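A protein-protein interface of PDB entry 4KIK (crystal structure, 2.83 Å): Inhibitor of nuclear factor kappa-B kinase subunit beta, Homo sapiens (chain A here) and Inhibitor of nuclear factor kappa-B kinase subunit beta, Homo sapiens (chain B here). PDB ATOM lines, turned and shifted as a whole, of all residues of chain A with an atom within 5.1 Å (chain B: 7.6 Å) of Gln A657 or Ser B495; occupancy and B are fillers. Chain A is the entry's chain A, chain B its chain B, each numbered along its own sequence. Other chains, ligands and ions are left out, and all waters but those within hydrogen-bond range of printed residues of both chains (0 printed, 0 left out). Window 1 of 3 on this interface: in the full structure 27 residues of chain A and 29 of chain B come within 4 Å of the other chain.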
ATOM      1  N   GLN A 653      -0.041 -22.434  -2.020  1.00  0.00           N
ATOM      2  CA  GLN A 653      -0.226 -23.309  -3.182  1.00  0.00           C
ATOM      3  C   GLN A 653      -1.712 -23.641  -3.370  1.00  0.00           C
ATOM      4  O   GLN A 653      -2.221 -23.538  -4.492  1.00  0.00           O
ATOM      5  CB  GLN A 653       0.613 -24.599  -3.046  1.00  0.00           C
ATOM      6  CG  GLN A 653       0.515 -25.551  -4.252  1.00  0.00           C
ATOM      7  CD  GLN A 653       1.221 -25.086  -5.506  1.00  0.00           C
ATOM      8  OE1 GLN A 653       2.035 -24.152  -5.493  1.00  0.00           O
ATOM      9  NE2 GLN A 653       0.931 -25.751  -6.623  1.00  0.00           N
ATOM     10  N   GLU A 654      -2.389 -24.023  -2.268  1.00  0.00           N
ATOM     11  CA  GLU A 654      -3.798 -24.364  -2.215  1.00  0.00           C
ATOM     12  C   GLU A 654      -4.628 -23.173  -2.675  1.00  0.00           C
ATOM     13  O   GLU A 654      -5.524 -23.349  -3.507  1.00  0.00           O
ATOM     14  CB  GLU A 654      -4.168 -24.796  -0.784  1.00  0.00           C
ATOM     15  CG  GLU A 654      -5.660 -24.843  -0.453  1.00  0.00           C
ATOM     16  CD  GLU A 654      -6.071 -25.393   0.908  1.00  0.00           C
ATOM     17  OE1 GLU A 654      -7.246 -25.805   1.039  1.00  0.00           O
ATOM     18  OE2 GLU A 654      -5.235 -25.403   1.843  1.00  0.00           O
ATOM     19  N   LYS A 655      -4.302 -21.960  -2.161  1.00  0.00           N
ATOM     20  CA  LYS A 655      -5.006 -20.711  -2.463  1.00  0.00           C
ATOM     21  C   LYS A 655      -4.895 -20.360  -3.942  1.00  0.00           C
ATOM     22  O   LYS A 655      -5.919 -20.068  -4.555  1.00  0.00           O
ATOM     23  CB  LYS A 655      -4.485 -19.558  -1.606  1.00  0.00           C
ATOM     24  CG  LYS A 655      -5.370 -18.317  -1.644  1.00  0.00           C
ATOM     25  CD  LYS A 655      -4.630 -17.108  -1.077  1.00  0.00           C
ATOM     26  CE  LYS A 655      -5.489 -15.885  -0.962  1.00  0.00           C
ATOM     27  NZ  LYS A 655      -4.736 -14.768  -0.348  1.00  0.00           N
ATOM     28  N   ARG A 656      -3.677 -20.429  -4.520  1.00  0.00           N
ATOM     29  CA  ARG A 656      -3.446 -20.133  -5.935  1.00  0.00           C
ATOM     30  C   ARG A 656      -4.251 -21.063  -6.828  1.00  0.00           C
ATOM     31  O   ARG A 656      -4.894 -20.584  -7.764  1.00  0.00           O
ATOM     32  CB  ARG A 656      -1.965 -20.226  -6.274  1.00  0.00           C
ATOM     33  CG  ARG A 656      -1.624 -19.477  -7.528  1.00  0.00           C
ATOM     34  CD  ARG A 656      -0.127 -19.341  -7.765  1.00  0.00           C
ATOM     35  NE  ARG A 656       0.470 -20.623  -8.151  1.00  0.00           N
ATOM     36  CZ  ARG A 656       1.214 -21.372  -7.346  1.00  0.00           C
ATOM     37  NH1 ARG A 656       1.505 -20.958  -6.124  1.00  0.00           N
ATOM     38  NH2 ARG A 656       1.685 -22.531  -7.763  1.00  0.00           N
ATOM     39  N   GLN A 657      -4.245 -22.382  -6.516  1.00  0.00           N
ATOM     40  CA  GLN A 657      -4.974 -23.417  -7.261  1.00  0.00           C
ATOM     41  C   GLN A 657      -6.473 -23.139  -7.219  1.00  0.00           C
ATOM     42  O   GLN A 657      -7.141 -23.208  -8.254  1.00  0.00           O
ATOM     43  CB  GLN A 657      -4.672 -24.813  -6.702  1.00  0.00           C
ATOM     44  CG  GLN A 657      -3.304 -25.346  -7.107  1.00  0.00           C
ATOM     45  CD  GLN A 657      -3.090 -26.806  -6.778  1.00  0.00           C
ATOM     46  OE1 GLN A 657      -2.087 -27.184  -6.195  1.00  0.00           O
ATOM     47  NE2 GLN A 657      -4.011 -27.664  -7.158  1.00  0.00           N
ATOM     48  N   LYS A 658      -6.986 -22.766  -6.033  1.00  0.00           N
ATOM     49  CA  LYS A 658      -8.401 -22.463  -5.840  1.00  0.00           C
ATOM     50  C   LYS A 658      -8.777 -21.170  -6.588  1.00  0.00           C
ATOM     51  O   LYS A 658      -9.886 -21.083  -7.127  1.00  0.00           O
ATOM     52  CB  LYS A 658      -8.754 -22.413  -4.341  1.00  0.00           C
ATOM     53  CG  LYS A 658      -8.838 -23.819  -3.727  1.00  0.00           C
ATOM     54  CD  LYS A 658      -9.293 -23.873  -2.275  1.00  0.00           C
ATOM     55  CE  LYS A 658      -9.472 -25.327  -1.859  1.00  0.00           C
ATOM     56  NZ  LYS A 658     -10.025 -25.500  -0.495  1.00  0.00           N
ATOM     57  N   GLU A 659      -7.827 -20.203  -6.676  1.00  0.00           N
ATOM     58  CA  GLU A 659      -7.992 -18.931  -7.400  1.00  0.00           C
ATOM     59  C   GLU A 659      -7.992 -19.179  -8.923  1.00  0.00           C
ATOM     60  O   GLU A 659      -8.662 -18.460  -9.657  1.00  0.00           O
ATOM     61  CB  GLU A 659      -6.905 -17.922  -7.020  1.00  0.00           C
ATOM     62  CG  GLU A 659      -7.149 -17.191  -5.703  1.00  0.00           C
ATOM     63  CD  GLU A 659      -5.993 -16.376  -5.127  1.00  0.00           C
ATOM     64  OE1 GLU A 659      -4.828 -16.617  -5.519  1.00  0.00           O
ATOM     65  OE2 GLU A 659      -6.250 -15.498  -4.269  1.00  0.00           O
ATOM     66  N   LEU A 660      -7.274 -20.210  -9.398  1.00  0.00           N
ATOM     67  CA  LEU A 660      -7.269 -20.558 -10.820  1.00  0.00           C
ATOM     68  C   LEU A 660      -8.611 -21.167 -11.221  1.00  0.00           C
ATOM     69  O   LEU A 660      -9.147 -20.769 -12.246  1.00  0.00           O
ATOM     70  CB  LEU A 660      -6.099 -21.503 -11.175  1.00  0.00           C
ATOM     71  CG  LEU A 660      -5.877 -21.868 -12.662  1.00  0.00           C
ATOM     72  CD1 LEU A 660      -5.975 -20.655 -13.581  1.00  0.00           C
ATOM     73  CD2 LEU A 660      -4.538 -22.498 -12.862  1.00  0.00           C
ATOM     74  N   TRP A 661      -9.174 -22.079 -10.403  1.00  0.00           N
ATOM     75  CA  TRP A 661     -10.486 -22.693 -10.643  1.00  0.00           C
ATOM     76  C   TRP A 661     -11.585 -21.649 -10.592  1.00  0.00           C
ATOM     77  O   TRP A 661     -12.638 -21.823 -11.218  1.00  0.00           O
ATOM     78  CB  TRP A 661     -10.773 -23.799  -9.628  1.00  0.00           C
ATOM     79  CG  TRP A 661     -10.060 -25.066  -9.938  1.00  0.00           C
ATOM     80  CD1 TRP A 661      -8.926 -25.532  -9.344  1.00  0.00           C
ATOM     81  CD2 TRP A 661     -10.395 -26.005 -10.965  1.00  0.00           C
ATOM     82  NE1 TRP A 661      -8.541 -26.718  -9.923  1.00  0.00           N
ATOM     83  CE2 TRP A 661      -9.429 -27.033 -10.925  1.00  0.00           C
ATOM     84  CE3 TRP A 661     -11.412 -26.070 -11.935  1.00  0.00           C
ATOM     85  CZ2 TRP A 661      -9.447 -28.115 -11.820  1.00  0.00           C
ATOM     86  CZ3 TRP A 661     -11.433 -27.147 -12.814  1.00  0.00           C
ATOM     87  CH2 TRP A 661     -10.453 -28.147 -12.759  1.00  0.00           C
ATOM     88  N   LYS B 488       8.076 -33.934  -2.409  1.00  0.00           N
ATOM     89  CA  LYS B 488       7.475 -33.619  -3.709  1.00  0.00           C
ATOM     90  C   LYS B 488       6.228 -34.479  -3.947  1.00  0.00           C
ATOM     91  O   LYS B 488       5.231 -33.961  -4.428  1.00  0.00           O
ATOM     92  CB  LYS B 488       8.482 -33.793  -4.848  1.00  0.00           C
ATOM     93  CG  LYS B 488       9.582 -32.747  -4.904  1.00  0.00           C
ATOM     94  CD  LYS B 488      10.492 -33.015  -6.127  1.00  0.00           C
ATOM     95  CE  LYS B 488      11.728 -32.148  -6.192  1.00  0.00           C
ATOM     96  NZ  LYS B 488      11.420 -30.747  -6.586  1.00  0.00           N
ATOM     97  N   LEU B 489       6.257 -35.758  -3.550  1.00  0.00           N
ATOM     98  CA  LEU B 489       5.105 -36.660  -3.685  1.00  0.00           C
ATOM     99  C   LEU B 489       3.919 -36.199  -2.861  1.00  0.00           C
ATOM    100  O   LEU B 489       2.792 -36.224  -3.351  1.00  0.00           O
ATOM    101  CB  LEU B 489       5.473 -38.076  -3.276  1.00  0.00           C
ATOM    102  CG  LEU B 489       6.267 -38.849  -4.273  1.00  0.00           C
ATOM    103  CD1 LEU B 489       6.886 -40.026  -3.607  1.00  0.00           C
ATOM    104  CD2 LEU B 489       5.393 -39.286  -5.438  1.00  0.00           C
ATOM    105  N   ASP B 490       4.190 -35.768  -1.616  1.00  0.00           N
ATOM    106  CA  ASP B 490       3.220 -35.226  -0.675  1.00  0.00           C
ATOM    107  C   ASP B 490       2.522 -34.020  -1.297  1.00  0.00           C
ATOM    108  O   ASP B 490       1.299 -33.943  -1.285  1.00  0.00           O
ATOM    109  CB  ASP B 490       3.955 -34.822   0.600  1.00  0.00           C
ATOM    110  CG  ASP B 490       3.102 -34.627   1.834  1.00  0.00           C
ATOM    111  OD1 ASP B 490       2.235 -33.712   1.827  1.00  0.00           O
ATOM    112  OD2 ASP B 490       3.394 -35.283   2.860  1.00  0.00           O
ATOM    113  N   PHE B 491       3.311 -33.125  -1.897  1.00  0.00           N
ATOM    114  CA  PHE B 491       2.888 -31.903  -2.544  1.00  0.00           C
ATOM    115  C   PHE B 491       2.033 -32.223  -3.768  1.00  0.00           C
ATOM    116  O   PHE B 491       0.975 -31.614  -3.917  1.00  0.00           O
ATOM    117  CB  PHE B 491       4.150 -31.095  -2.886  1.00  0.00           C
ATOM    118  CG  PHE B 491       4.057 -29.874  -3.763  1.00  0.00           C
ATOM    119  CD1 PHE B 491       4.270 -28.599  -3.234  1.00  0.00           C
ATOM    120  CD2 PHE B 491       3.823 -29.998  -5.143  1.00  0.00           C
ATOM    121  CE1 PHE B 491       4.205 -27.463  -4.063  1.00  0.00           C
ATOM    122  CE2 PHE B 491       3.726 -28.870  -5.961  1.00  0.00           C
ATOM    123  CZ  PHE B 491       3.930 -27.607  -5.421  1.00  0.00           C
ATOM    124  N   PHE B 492       2.493 -33.133  -4.645  1.00  0.00           N
ATOM    125  CA  PHE B 492       1.752 -33.539  -5.842  1.00  0.00           C
ATOM    126  C   PHE B 492       0.422 -34.159  -5.453  1.00  0.00           C
ATOM    127  O   PHE B 492      -0.593 -33.856  -6.079  1.00  0.00           O
ATOM    128  CB  PHE B 492       2.561 -34.547  -6.691  1.00  0.00           C
ATOM    129  CG  PHE B 492       1.892 -35.021  -7.976  1.00  0.00           C
ATOM    130  CD1 PHE B 492       2.185 -34.421  -9.198  1.00  0.00           C
ATOM    131  CD2 PHE B 492       0.986 -36.077  -7.965  1.00  0.00           C
ATOM    132  CE1 PHE B 492       1.575 -34.863 -10.383  1.00  0.00           C
ATOM    133  CE2 PHE B 492       0.359 -36.498  -9.149  1.00  0.00           C
ATOM    134  CZ  PHE B 492       0.683 -35.912 -10.353  1.00  0.00           C
ATOM    135  N   LYS B 493       0.434 -35.042  -4.434  1.00  0.00           N
ATOM    136  CA  LYS B 493      -0.765 -35.726  -3.944  1.00  0.00           C
ATOM    137  C   LYS B 493      -1.792 -34.693  -3.442  1.00  0.00           C
ATOM    138  O   LYS B 493      -2.983 -34.803  -3.758  1.00  0.00           O
ATOM    139  CB  LYS B 493      -0.400 -36.763  -2.860  1.00  0.00           C
ATOM    140  CG  LYS B 493      -0.064 -38.121  -3.457  1.00  0.00           C
ATOM    141  CD  LYS B 493       0.906 -38.972  -2.644  1.00  0.00           C
ATOM    142  CE  LYS B 493       1.298 -40.172  -3.488  1.00  0.00           C
ATOM    143  NZ  LYS B 493       2.178 -41.140  -2.781  1.00  0.00           N
ATOM    144  N   THR B 494      -1.302 -33.639  -2.756  1.00  0.00           N
ATOM    145  CA  THR B 494      -2.113 -32.532  -2.270  1.00  0.00           C
ATOM    146  C   THR B 494      -2.663 -31.743  -3.474  1.00  0.00           C
ATOM    147  O   THR B 494      -3.873 -31.546  -3.585  1.00  0.00           O
ATOM    148  CB  THR B 494      -1.275 -31.679  -1.306  1.00  0.00           C
ATOM    149  OG1 THR B 494      -1.055 -32.444  -0.112  1.00  0.00           O
ATOM    150  CG2 THR B 494      -1.938 -30.338  -0.956  1.00  0.00           C
ATOM    151  N   SER B 495      -1.771 -31.329  -4.381  1.00  0.00           N
ATOM    152  CA  SER B 495      -2.108 -30.553  -5.565  1.00  0.00           C
ATOM    153  C   SER B 495      -3.208 -31.227  -6.413  1.00  0.00           C
ATOM    154  O   SER B 495      -4.284 -30.635  -6.595  1.00  0.00           O
ATOM    155  CB  SER B 495      -0.858 -30.313  -6.392  1.00  0.00           C
ATOM    156  OG  SER B 495      -1.103 -29.325  -7.374  1.00  0.00           O
ATOM    157  N   ILE B 496      -2.975 -32.491  -6.851  1.00  0.00           N
ATOM    158  CA  ILE B 496      -3.918 -33.254  -7.671  1.00  0.00           C
ATOM    159  C   ILE B 496      -5.247 -33.485  -6.957  1.00  0.00           C
ATOM    160  O   ILE B 496      -6.273 -33.447  -7.622  1.00  0.00           O
ATOM    161  CB  ILE B 496      -3.316 -34.572  -8.183  1.00  0.00           C
ATOM    162  CG1 ILE B 496      -4.080 -35.058  -9.443  1.00  0.00           C
ATOM    163  CG2 ILE B 496      -3.184 -35.656  -7.076  1.00  0.00           C
ATOM    164  CD1 ILE B 496      -3.291 -35.940 -10.378  1.00  0.00           C
ATOM    165  N   GLN B 497      -5.250 -33.684  -5.630  1.00  0.00           N
ATOM    166  CA  GLN B 497      -6.492 -33.905  -4.896  1.00  0.00           C
ATOM    167  C   GLN B 497      -7.395 -32.640  -4.983  1.00  0.00           C
ATOM    168  O   GLN B 497      -8.596 -32.782  -5.230  1.00  0.00           O
ATOM    169  CB  GLN B 497      -6.201 -34.333  -3.439  1.00  0.00           C
ATOM    170  CG  GLN B 497      -7.425 -34.467  -2.504  1.00  0.00           C
ATOM    171  CD  GLN B 497      -8.599 -35.304  -3.016  1.00  0.00           C
ATOM    172  OE1 GLN B 497      -9.767 -34.891  -2.915  1.00  0.00           O
ATOM    173  NE2 GLN B 497      -8.325 -36.471  -3.615  1.00  0.00           N
ATOM    174  N   ILE B 498      -6.801 -31.424  -4.876  1.00  0.00           N
ATOM    175  CA  ILE B 498      -7.519 -30.153  -5.019  1.00  0.00           C
ATOM    176  C   ILE B 498      -8.098 -30.069  -6.441  1.00  0.00           C
ATOM    177  O   ILE B 498      -9.305 -29.866  -6.610  1.00  0.00           O
ATOM    178  CB  ILE B 498      -6.622 -28.914  -4.703  1.00  0.00           C
ATOM    179  CG1 ILE B 498      -6.088 -28.955  -3.269  1.00  0.00           C
ATOM    180  CG2 ILE B 498      -7.361 -27.584  -4.976  1.00  0.00           C
ATOM    181  CD1 ILE B 498      -4.832 -28.201  -3.049  1.00  0.00           C
ATOM    182  N   ASP B 499      -7.229 -30.245  -7.452  1.00  0.00           N
ATOM    183  CA  ASP B 499      -7.598 -30.168  -8.860  1.00  0.00           C
ATOM    184  C   ASP B 499      -8.740 -31.146  -9.218  1.00  0.00           C
ATOM    185  O   ASP B 499      -9.649 -30.755  -9.958  1.00  0.00           O
ATOM    186  CB  ASP B 499      -6.354 -30.371  -9.747  1.00  0.00           C
ATOM    187  CG  ASP B 499      -5.436 -29.152  -9.763  1.00  0.00           C
ATOM    188  OD1 ASP B 499      -5.906 -28.045  -9.387  1.00  0.00           O
ATOM    189  OD2 ASP B 499      -4.258 -29.294 -10.188  1.00  0.00           O
ATOM    190  N   LEU B 500      -8.736 -32.374  -8.645  1.00  0.00           N
ATOM    191  CA  LEU B 500      -9.789 -33.376  -8.901  1.00  0.00           C
ATOM    192  C   LEU B 500     -11.100 -32.993  -8.218  1.00  0.00           C
ATOM    193  O   LEU B 500     -12.160 -33.168  -8.822  1.00  0.00           O
ATOM    194  CB  LEU B 500      -9.370 -34.783  -8.454  1.00  0.00           C
ATOM    195  CG  LEU B 500      -8.273 -35.466  -9.254  1.00  0.00           C
ATOM    196  CD1 LEU B 500      -7.569 -36.476  -8.411  1.00  0.00           C
ATOM    197  CD2 LEU B 500      -8.809 -36.093 -10.531  1.00  0.00           C
ATOM    198  N   GLU B 501     -11.022 -32.461  -6.971  1.00  0.00           N
ATOM    199  CA  GLU B 501     -12.176 -32.021  -6.182  1.00  0.00           C
ATOM    200  C   GLU B 501     -12.900 -30.835  -6.857  1.00  0.00           C
ATOM    201  O   GLU B 501     -14.098 -30.932  -7.140  1.00  0.00           O
ATOM    202  CB  GLU B 501     -11.721 -31.633  -4.776  1.00  0.00           C
ATOM    203  CG  GLU B 501     -12.753 -31.836  -3.689  1.00  0.00           C
ATOM    204  CD  GLU B 501     -12.329 -31.201  -2.381  1.00  0.00           C
ATOM    205  OE1 GLU B 501     -11.474 -31.793  -1.684  1.00  0.00           O
ATOM    206  OE2 GLU B 501     -12.808 -30.085  -2.079  1.00  0.00           O
ATOM    207  N   LYS B 502     -12.154 -29.749  -7.167  1.00  0.00           N
ATOM    208  CA  LYS B 502     -12.697 -28.535  -7.775  1.00  0.00           C
ATOM    209  C   LYS B 502     -13.188 -28.751  -9.224  1.00  0.00           C
ATOM    210  O   LYS B 502     -14.040 -27.974  -9.669  1.00  0.00           O
ATOM    211  CB  LYS B 502     -11.693 -27.383  -7.686  1.00  0.00           C
ATOM    212  CG  LYS B 502     -11.409 -26.954  -6.230  1.00  0.00           C
ATOM    213  CD  LYS B 502     -12.393 -25.904  -5.632  1.00  0.00           C
ATOM    214  CE  LYS B 502     -11.920 -24.467  -5.877  1.00  0.00           C
ATOM    215  NZ  LYS B 502     -12.708 -23.404  -5.182  1.00  0.00           N
ATOM    216  N   GLN B 653       2.945 -32.900 -13.025  1.00  0.00           N
ATOM    217  CA  GLN B 653       2.487 -31.676 -12.391  1.00  0.00           C
ATOM    218  C   GLN B 653       2.407 -30.552 -13.421  1.00  0.00           C
ATOM    219  O   GLN B 653       1.410 -29.826 -13.452  1.00  0.00           O
ATOM    220  CB  GLN B 653       3.406 -31.282 -11.223  1.00  0.00           C
ATOM    221  CG  GLN B 653       2.960 -30.006 -10.460  1.00  0.00           C
ATOM    222  CD  GLN B 653       1.737 -30.182  -9.584  1.00  0.00           C
ATOM    223  OE1 GLN B 653       1.282 -31.291  -9.295  1.00  0.00           O
ATOM    224  NE2 GLN B 653       1.183 -29.087  -9.123  1.00  0.00           N
ATOM    225  N   ARG B 656      -0.554 -31.191 -15.924  1.00  0.00           N
ATOM    226  CA  ARG B 656      -1.854 -30.893 -15.322  1.00  0.00           C
ATOM    227  C   ARG B 656      -2.124 -29.386 -15.269  1.00  0.00           C
ATOM    228  O   ARG B 656      -3.208 -28.949 -15.668  1.00  0.00           O
ATOM    229  CB  ARG B 656      -1.956 -31.501 -13.921  1.00  0.00           C
ATOM    230  CG  ARG B 656      -3.390 -31.636 -13.444  1.00  0.00           C
ATOM    231  CD  ARG B 656      -3.537 -32.460 -12.189  1.00  0.00           C
ATOM    232  NE  ARG B 656      -3.055 -31.721 -11.033  1.00  0.00           N
ATOM    233  CZ  ARG B 656      -1.906 -31.974 -10.424  1.00  0.00           C
ATOM    234  NH1 ARG B 656      -1.140 -32.975 -10.829  1.00  0.00           N
ATOM    235  NH2 ARG B 656      -1.527 -31.243  -9.394  1.00  0.00           N
ATOM    236  N   GLN B 657      -1.121 -28.600 -14.826  1.00  0.00           N
ATOM    237  CA  GLN B 657      -1.182 -27.145 -14.714  1.00  0.00           C
ATOM    238  C   GLN B 657      -1.430 -26.522 -16.064  1.00  0.00           C
ATOM    239  O   GLN B 657      -2.303 -25.657 -16.182  1.00  0.00           O
ATOM    240  CB  GLN B 657       0.111 -26.592 -14.105  1.00  0.00           C
ATOM    241  CG  GLN B 657       0.216 -26.825 -12.602  1.00  0.00           C
ATOM    242  CD  GLN B 657       1.318 -26.046 -11.932  1.00  0.00           C
ATOM    243  OE1 GLN B 657       2.103 -26.594 -11.154  1.00  0.00           O
ATOM    244  NE2 GLN B 657       1.359 -24.737 -12.158  1.00  0.00           N
ATOM    245  N   LEU B 660      -4.973 -27.159 -17.234  1.00  0.00           N
ATOM    246  CA  LEU B 660      -5.945 -26.304 -16.570  1.00  0.00           C
ATOM    247  C   LEU B 660      -5.992 -24.931 -17.252  1.00  0.00           C
ATOM    248  O   LEU B 660      -7.090 -24.432 -17.490  1.00  0.00           O
ATOM    249  CB  LEU B 660      -5.633 -26.184 -15.067  1.00  0.00           C
ATOM    250  CG  LEU B 660      -6.652 -25.437 -14.177  1.00  0.00           C
ATOM    251  CD1 LEU B 660      -8.117 -25.827 -14.484  1.00  0.00           C
ATOM    252  CD2 LEU B 660      -6.358 -25.674 -12.699  1.00  0.00           C
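Of the 9 printed residues of chain A, 5 touch a printed residue of chain B.
Hydrophobic or aromatic side chains of chain A that line the printed part of chain B: Leu A660 and Trp A661.
Of the 19 printed residues of chain B, 6 touch a printed residue of chain A.
Hydrophobic or aromatic side chains of chain B within 4 Å of the printed part of chain A: Phe B491, Ile B498 and Leu B660.
Among the printed residues, 9 pairs touch across the chains.
Among the printed residues, no Asp or Glu carboxylate lies within 4 Å of a Lys or Arg side-chain nitrogen of the other chain.
Among the printed residues, pairs that only touch across the chains: Gln A653 with Phe B491 (3.7 Å), Gln A657 with Ile B498 (3.8 Å), Lys A658 with Lys B502 (3.8 Å), Leu A660 with Leu B660 (3.7 Å), Trp A661 with Lys B502 (3.6 Å) and Trp A661 with Leu B660 (3.7 Å).
Gln A657 touches three residues of chain B.
Of the printed residues of chain B, Trp A661 touches Asp B499, Lys B502 and Leu B660.
Printed residues of chain A within 4 Å of Phe B491: Gln A653 (3.7 Å).
Printed residues of chain A within 4 Å of Lys B502: Lys A658 (3.8 Å) and Trp A661 (3.6 Å).
Of the printed residues of chain B, Leu A660 touches Leu B660 (3.7 Å).
Of the printed residues of chain B, Gln A653 touches Phe B491.
The nearest residue of chain B that does not touch Gln A657 is Gln B653 (4.8 Å).
The nearest printed residue of chain A that does not touch Ile B498 is Glu A654 (4.1 Å).
OE1 of Gln A653 is in hydrogen-bond range of NH2 of Arg A656 (2.8 Å).
The side-chain hydroxyl (OG) of Ser B495 lies within hydrogen-bond range of the guanidinium group (NH2) of Arg B656 (2.8 Å).
The side-chain carboxylate of Asp B499 is in salt-bridge range of the guanidinium group of Arg B656, 2.8 Å away.
The side-chain amino group of Lys A658 is in salt-bridge range of the side-chain carboxylate of Glu A654, 3.2 Å away.
NE2 of Gln B653 lies within hydrogen-bond range of OG of Ser B495, 2.9 Å away.
The side-chain amide oxygen (OE1) of Gln A657 is in hydrogen-bond range of the side-chain amide nitrogen (NE2) of Gln A653 (3.4 Å).
NE1 of Trp A661 is in hydrogen-bond range of OD1 of Asp B499 (3.0 Å).
OG of Ser B495 lies within hydrogen-bond range of OE1 of Gln A657 (2.6 Å).
The side-chain amide nitrogen (NE2) of Gln A657 sits at hydrogen-bond distance from the side-chain carboxylate (OD1) of Asp B499 (3.0 Å).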
